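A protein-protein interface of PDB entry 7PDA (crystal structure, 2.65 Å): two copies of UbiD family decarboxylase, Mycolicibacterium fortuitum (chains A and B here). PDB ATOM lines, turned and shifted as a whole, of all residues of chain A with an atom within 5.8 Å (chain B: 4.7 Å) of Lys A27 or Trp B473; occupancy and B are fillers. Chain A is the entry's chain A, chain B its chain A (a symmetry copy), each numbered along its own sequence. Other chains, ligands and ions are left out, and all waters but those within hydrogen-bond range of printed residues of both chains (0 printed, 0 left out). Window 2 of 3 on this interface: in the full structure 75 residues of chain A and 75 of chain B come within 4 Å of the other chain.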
ATOM      1  N   THR A  25      22.640   4.739  30.682  1.00  0.00           N
ATOM      2  CA  THR A  25      22.865   6.141  30.398  1.00  0.00           C
ATOM      3  C   THR A  25      23.056   6.371  28.897  1.00  0.00           C
ATOM      4  O   THR A  25      23.893   5.725  28.257  1.00  0.00           O
ATOM      5  CB  THR A  25      24.135   6.597  31.107  1.00  0.00           C
ATOM      6  OG1 THR A  25      23.789   6.347  32.464  1.00  0.00           O
ATOM      7  CG2 THR A  25      24.457   8.054  30.865  1.00  0.00           C
ATOM      8  N   ILE A  26      22.277   7.307  28.341  1.00  0.00           N
ATOM      9  CA  ILE A  26      22.271   7.516  26.902  1.00  0.00           C
ATOM     10  C   ILE A  26      22.865   8.891  26.625  1.00  0.00           C
ATOM     11  O   ILE A  26      22.351   9.888  27.146  1.00  0.00           O
ATOM     12  CB  ILE A  26      20.845   7.415  26.335  1.00  0.00           C
ATOM     13  CG1 ILE A  26      20.156   6.080  26.645  1.00  0.00           C
ATOM     14  CG2 ILE A  26      20.836   7.742  24.851  1.00  0.00           C
ATOM     15  CD1 ILE A  26      20.867   4.831  26.163  1.00  0.00           C
ATOM     16  N   LYS A  27      23.911   8.917  25.782  1.00  0.00           N
ATOM     17  CA  LYS A  27      24.653  10.133  25.471  1.00  0.00           C
ATOM     18  C   LYS A  27      24.342  10.625  24.050  1.00  0.00           C
ATOM     19  O   LYS A  27      24.298   9.842  23.094  1.00  0.00           O
ATOM     20  CB  LYS A  27      26.136   9.876  25.748  1.00  0.00           C
ATOM     21  CG  LYS A  27      26.519   9.857  27.224  1.00  0.00           C
ATOM     22  CD  LYS A  27      27.911   9.376  27.542  1.00  0.00           C
ATOM     23  CE  LYS A  27      28.088   9.269  29.041  1.00  0.00           C
ATOM     24  NZ  LYS A  27      29.523   9.257  29.392  1.00  0.00           N
ATOM     25  N   GLY A  28      24.041  11.926  23.932  1.00  0.00           N
ATOM     26  CA  GLY A  28      23.872  12.600  22.645  1.00  0.00           C
ATOM     27  C   GLY A  28      22.529  12.344  21.945  1.00  0.00           C
ATOM     28  O   GLY A  28      22.417  12.524  20.739  1.00  0.00           O
ATOM     29  N   ALA A  29      21.474  11.957  22.661  1.00  0.00           N
ATOM     30  CA  ALA A  29      20.162  12.137  22.055  1.00  0.00           C
ATOM     31  C   ALA A  29      19.664  13.573  22.283  1.00  0.00           C
ATOM     32  O   ALA A  29      19.996  14.191  23.304  1.00  0.00           O
ATOM     33  CB  ALA A  29      19.188  11.113  22.582  1.00  0.00           C
ATOM     34  N   GLU A  34      13.666  13.215  19.684  1.00  0.00           N
ATOM     35  CA  GLU A  34      14.541  12.065  19.682  1.00  0.00           C
ATOM     36  C   GLU A  34      14.487  11.292  21.004  1.00  0.00           C
ATOM     37  O   GLU A  34      14.328  10.077  20.972  1.00  0.00           O
ATOM     38  CB  GLU A  34      15.952  12.462  19.316  1.00  0.00           C
ATOM     39  CG  GLU A  34      16.810  11.262  19.029  1.00  0.00           C
ATOM     40  CD  GLU A  34      18.224  11.617  18.630  1.00  0.00           C
ATOM     41  OE1 GLU A  34      18.851  10.729  18.008  1.00  0.00           O
ATOM     42  OE2 GLU A  34      18.701  12.764  18.961  1.00  0.00           O
ATOM     43  N   ILE A  38      12.865   7.453  21.509  1.00  0.00           N
ATOM     44  CA  ILE A  38      13.649   6.401  22.143  1.00  0.00           C
ATOM     45  C   ILE A  38      12.896   5.818  23.347  1.00  0.00           C
ATOM     46  O   ILE A  38      12.839   4.602  23.501  1.00  0.00           O
ATOM     47  CB  ILE A  38      15.020   6.916  22.585  1.00  0.00           C
ATOM     48  CG1 ILE A  38      15.979   7.166  21.419  1.00  0.00           C
ATOM     49  CG2 ILE A  38      15.630   5.973  23.615  1.00  0.00           C
ATOM     50  CD1 ILE A  38      17.131   8.097  21.796  1.00  0.00           C
ATOM     51  N   LEU A  51      18.447   6.941  31.308  1.00  0.00           N
ATOM     52  CA  LEU A  51      19.035   8.139  31.895  1.00  0.00           C
ATOM     53  C   LEU A  51      19.769   8.917  30.797  1.00  0.00           C
ATOM     54  O   LEU A  51      20.809   8.484  30.301  1.00  0.00           O
ATOM     55  CB  LEU A  51      19.958   7.703  33.042  1.00  0.00           C
ATOM     56  CG  LEU A  51      20.610   8.825  33.866  1.00  0.00           C
ATOM     57  CD1 LEU A  51      19.593   9.842  34.393  1.00  0.00           C
ATOM     58  CD2 LEU A  51      21.479   8.258  34.986  1.00  0.00           C
ATOM     59  N   PHE A  52      19.182  10.035  30.367  1.00  0.00           N
ATOM     60  CA  PHE A  52      19.652  10.744  29.171  1.00  0.00           C
ATOM     61  C   PHE A  52      20.665  11.806  29.579  1.00  0.00           C
ATOM     62  O   PHE A  52      20.348  12.688  30.383  1.00  0.00           O
ATOM     63  CB  PHE A  52      18.496  11.312  28.315  1.00  0.00           C
ATOM     64  CG  PHE A  52      17.646  10.255  27.644  1.00  0.00           C
ATOM     65  CD1 PHE A  52      17.932   9.820  26.358  1.00  0.00           C
ATOM     66  CD2 PHE A  52      16.585   9.665  28.315  1.00  0.00           C
ATOM     67  CE1 PHE A  52      17.181   8.815  25.764  1.00  0.00           C
ATOM     68  CE2 PHE A  52      15.845   8.652  27.725  1.00  0.00           C
ATOM     69  CZ  PHE A  52      16.153   8.213  26.458  1.00  0.00           C
ATOM     70  N   ASP A  53      21.869  11.689  29.004  1.00  0.00           N
ATOM     71  CA  ASP A  53      22.952  12.625  29.294  1.00  0.00           C
ATOM     72  C   ASP A  53      23.551  13.260  28.039  1.00  0.00           C
ATOM     73  O   ASP A  53      23.298  12.839  26.905  1.00  0.00           O
ATOM     74  CB  ASP A  53      24.063  11.976  30.109  1.00  0.00           C
ATOM     75  CG  ASP A  53      24.652  12.962  31.095  1.00  0.00           C
ATOM     76  OD1 ASP A  53      24.309  14.169  31.008  1.00  0.00           O
ATOM     77  OD2 ASP A  53      25.437  12.519  31.947  1.00  0.00           O
ATOM     78  N   ASP A  54      24.396  14.272  28.275  1.00  0.00           N
ATOM     79  CA  ASP A  54      25.101  14.995  27.224  1.00  0.00           C
ATOM     80  C   ASP A  54      24.111  15.287  26.110  1.00  0.00           C
ATOM     81  O   ASP A  54      24.272  14.841  24.975  1.00  0.00           O
ATOM     82  CB  ASP A  54      26.256  14.192  26.620  1.00  0.00           C
ATOM     83  CG  ASP A  54      27.423  14.002  27.557  1.00  0.00           C
ATOM     84  OD1 ASP A  54      27.718  14.956  28.299  1.00  0.00           O
ATOM     85  OD2 ASP A  54      28.017  12.897  27.526  1.00  0.00           O
ATOM     86  N   ILE B 469      15.168   6.395  14.268  1.00  0.00           N
ATOM     87  CA  ILE B 469      15.765   6.243  15.582  1.00  0.00           C
ATOM     88  C   ILE B 469      16.225   4.796  15.804  1.00  0.00           C
ATOM     89  O   ILE B 469      17.283   4.572  16.372  1.00  0.00           O
ATOM     90  CB  ILE B 469      14.787   6.761  16.656  1.00  0.00           C
ATOM     91  CG1 ILE B 469      14.356   8.212  16.404  1.00  0.00           C
ATOM     92  CG2 ILE B 469      15.374   6.589  18.040  1.00  0.00           C
ATOM     93  CD1 ILE B 469      15.488   9.230  16.160  1.00  0.00           C
ATOM     94  N   ARG B 470      15.452   3.810  15.347  1.00  0.00           N
ATOM     95  CA  ARG B 470      15.805   2.408  15.581  1.00  0.00           C
ATOM     96  C   ARG B 470      17.178   2.079  14.963  1.00  0.00           C
ATOM     97  O   ARG B 470      18.101   1.592  15.626  1.00  0.00           O
ATOM     98  CB  ARG B 470      14.666   1.507  15.079  1.00  0.00           C
ATOM     99  CG  ARG B 470      14.732   0.055  15.528  1.00  0.00           C
ATOM    100  CD  ARG B 470      13.498  -0.744  15.094  1.00  0.00           C
ATOM    101  NE  ARG B 470      12.226  -0.006  14.952  1.00  0.00           N
ATOM    102  CZ  ARG B 470      11.313   0.216  15.916  1.00  0.00           C
ATOM    103  NH1 ARG B 470      11.519  -0.201  17.162  1.00  0.00           N
ATOM    104  NH2 ARG B 470      10.203   0.886  15.632  1.00  0.00           N
ATOM    105  N   ASP B 471      17.313   2.374  13.670  1.00  0.00           N
ATOM    106  CA  ASP B 471      18.512   2.077  12.910  1.00  0.00           C
ATOM    107  C   ASP B 471      19.631   3.060  13.270  1.00  0.00           C
ATOM    108  O   ASP B 471      20.795   2.769  13.025  1.00  0.00           O
ATOM    109  CB  ASP B 471      18.159   1.922  11.424  1.00  0.00           C
ATOM    110  CG  ASP B 471      19.173   2.504  10.450  1.00  0.00           C
ATOM    111  OD1 ASP B 471      20.362   2.098  10.516  1.00  0.00           O
ATOM    112  OD2 ASP B 471      18.757   3.349   9.616  1.00  0.00           O
ATOM    113  N   ARG B 472      19.296   4.209  13.874  1.00  0.00           N
ATOM    114  CA  ARG B 472      20.341   5.096  14.356  1.00  0.00           C
ATOM    115  C   ARG B 472      20.870   4.654  15.715  1.00  0.00           C
ATOM    116  O   ARG B 472      22.056   4.766  15.927  1.00  0.00           O
ATOM    117  CB  ARG B 472      19.895   6.555  14.467  1.00  0.00           C
ATOM    118  CG  ARG B 472      21.075   7.507  14.614  1.00  0.00           C
ATOM    119  CD  ARG B 472      20.974   8.356  15.850  1.00  0.00           C
ATOM    120  NE  ARG B 472      19.931   9.313  15.568  1.00  0.00           N
ATOM    121  CZ  ARG B 472      20.170  10.542  15.148  1.00  0.00           C
ATOM    122  NH1 ARG B 472      21.434  10.943  15.011  1.00  0.00           N
ATOM    123  NH2 ARG B 472      19.140  11.353  14.906  1.00  0.00           N
ATOM    124  N   TRP B 473      20.010   4.194  16.634  1.00  0.00           N
ATOM    125  CA  TRP B 473      20.429   3.771  17.966  1.00  0.00           C
ATOM    126  C   TRP B 473      20.615   2.248  18.073  1.00  0.00           C
ATOM    127  O   TRP B 473      20.378   1.671  19.139  1.00  0.00           O
ATOM    128  CB  TRP B 473      19.466   4.319  19.021  1.00  0.00           C
ATOM    129  CG  TRP B 473      19.659   5.791  19.209  1.00  0.00           C
ATOM    130  CD1 TRP B 473      18.997   6.812  18.580  1.00  0.00           C
ATOM    131  CD2 TRP B 473      20.627   6.416  20.064  1.00  0.00           C
ATOM    132  NE1 TRP B 473      19.461   8.027  19.012  1.00  0.00           N
ATOM    133  CE2 TRP B 473      20.463   7.813  19.923  1.00  0.00           C
ATOM    134  CE3 TRP B 473      21.572   5.934  20.972  1.00  0.00           C
ATOM    135  CZ2 TRP B 473      21.218   8.723  20.656  1.00  0.00           C
ATOM    136  CZ3 TRP B 473      22.337   6.838  21.672  1.00  0.00           C
ATOM    137  CH2 TRP B 473      22.174   8.216  21.505  1.00  0.00           C
ATOM    138  N   LYS B 474      21.150   1.632  16.992  1.00  0.00           N
ATOM    139  CA  LYS B 474      21.160   0.190  16.739  1.00  0.00           C
ATOM    140  C   LYS B 474      21.910  -0.580  17.829  1.00  0.00           C
ATOM    141  O   LYS B 474      21.293  -1.447  18.448  1.00  0.00           O
ATOM    142  CB  LYS B 474      21.635  -0.145  15.313  1.00  0.00           C
ATOM    143  CG  LYS B 474      21.069  -1.432  14.713  1.00  0.00           C
ATOM    144  CD  LYS B 474      21.896  -2.678  15.058  1.00  0.00           C
ATOM    145  CE  LYS B 474      21.288  -3.995  14.613  1.00  0.00           C
ATOM    146  NZ  LYS B 474      21.503  -5.053  15.630  1.00  0.00           N
ATOM    147  N   ALA B 475      23.198  -0.253  18.054  1.00  0.00           N
ATOM    148  CA  ALA B 475      24.112  -0.998  18.923  1.00  0.00           C
ATOM    149  C   ALA B 475      23.761  -0.864  20.415  1.00  0.00           C
ATOM    150  O   ALA B 475      23.322  -1.840  21.054  1.00  0.00           O
ATOM    151  CB  ALA B 475      25.537  -0.573  18.649  1.00  0.00           C
ATOM    152  N   THR B 476      24.066   0.333  20.954  1.00  0.00           N
ATOM    153  CA  THR B 476      23.554   1.004  22.155  1.00  0.00           C
ATOM    154  C   THR B 476      22.383   0.318  22.878  1.00  0.00           C
ATOM    155  O   THR B 476      22.502   0.091  24.079  1.00  0.00           O
ATOM    156  CB  THR B 476      23.164   2.463  21.863  1.00  0.00           C
ATOM    157  OG1 THR B 476      22.337   2.324  20.708  1.00  0.00           O
ATOM    158  CG2 THR B 476      24.335   3.378  21.563  1.00  0.00           C
ATOM    159  N   LEU B 477      21.246   0.064  22.205  1.00  0.00           N
ATOM    160  CA  LEU B 477      19.999  -0.192  22.917  1.00  0.00           C
ATOM    161  C   LEU B 477      19.123  -1.123  22.082  1.00  0.00           C
ATOM    162  O   LEU B 477      18.898  -0.809  20.912  1.00  0.00           O
ATOM    163  CB  LEU B 477      19.267   1.144  23.071  1.00  0.00           C
ATOM    164  CG  LEU B 477      18.483   1.397  24.357  1.00  0.00           C
ATOM    165  CD1 LEU B 477      17.771   2.739  24.272  1.00  0.00           C
ATOM    166  CD2 LEU B 477      17.484   0.280  24.644  1.00  0.00           C
ATOM    167  N   LEU B 479      15.789  -1.564  21.312  1.00  0.00           N
ATOM    168  CA  LEU B 479      14.808  -0.937  20.418  1.00  0.00           C
ATOM    169  C   LEU B 479      14.358  -1.888  19.290  1.00  0.00           C
ATOM    170  O   LEU B 479      13.661  -1.395  18.358  1.00  0.00           O
ATOM    171  CB  LEU B 479      15.337   0.366  19.806  1.00  0.00           C
ATOM    172  CG  LEU B 479      15.578   1.523  20.768  1.00  0.00           C
ATOM    173  CD1 LEU B 479      16.157   2.721  20.030  1.00  0.00           C
ATOM    174  CD2 LEU B 479      14.295   1.936  21.445  1.00  0.00           C
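Among the printed residues, pairs that only touch across the chains: Ile A26 with Trp B473, Lys A27 with Trp B473, Gly A28 with Trp B473, Ala A29 with Trp B473, Glu A34 with Ile B469, Ile A38 with Ile B469, Ile A38 with Trp B473, Ile A38 with Leu B477 and Ile A38 with Leu B479.
Of the 11 printed residues of chain A, 6 touch a printed residue of chain B. Hydrophobic or aromatic side chains of chain A within 4 Å of the printed part of chain B: Ile A26, Ala A29 and Ile A38. Hydrophobic or aromatic side chains of chain B within 4 Å of the printed part of chain A: Ile B469, Trp B473, Leu B477 and Leu B479. Among the printed residues, 11 pairs touch across the chains. Among the printed residues, Asp or Glu carboxylates within 4 Å of a Lys or Arg side-chain nitrogen of the other chain: Glu A34 with Arg B472.
The guanidinium group of Arg B472 lies within salt-bridge range of the side-chain carboxylate of Glu A34 (3.0 Å). The side-chain carboxylate of Glu A34 lies within hydrogen-bond range of the indole nitrogen of Trp B473 (2.9 Å).
N of Gly A28 sits at hydrogen-bond distance from O of Asp A54 (3.1 Å). O of Leu A51 lies within hydrogen-bond range of N of Ile A26 (2.7 Å). O of Leu B479 is in hydrogen-bond range of NH1 of Arg B470 (2.7 Å). N of Gly A28 sits at hydrogen-bond distance from O of Asp A53 (3.2 Å). The backbone carbonyl oxygen (O) of Trp B473 is in hydrogen-bond range of the side-chain hydroxyl (OG1) of Thr B476. The backbone carbonyl oxygen (O) of Ile A26 is in hydrogen-bond range of the backbone NH (N) of Asp A53, 2.6 Å away.
Printed residues of chain B within 4 Å of Gly A28: Trp B473 (3.99 Å). Printed residues of chain B within 4 Å of Ile A38: Ile B469, Trp B473, Leu B477 and Leu B479. Leu A51 touches none of the printed residues of chain B. Of the printed residues of chain A, Trp B473 touches Ile A26, Lys A27, Gly A28, Ala A29, Glu A34 and Ile A38. The nearest printed residue of chain A that does not touch Arg B472 is Gly A28 (6.0 Å).
No position is printed for both chains. Of the 11 pairs that touch across the chains among the printed residues, none has its exchanged pair printed and touching as well.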
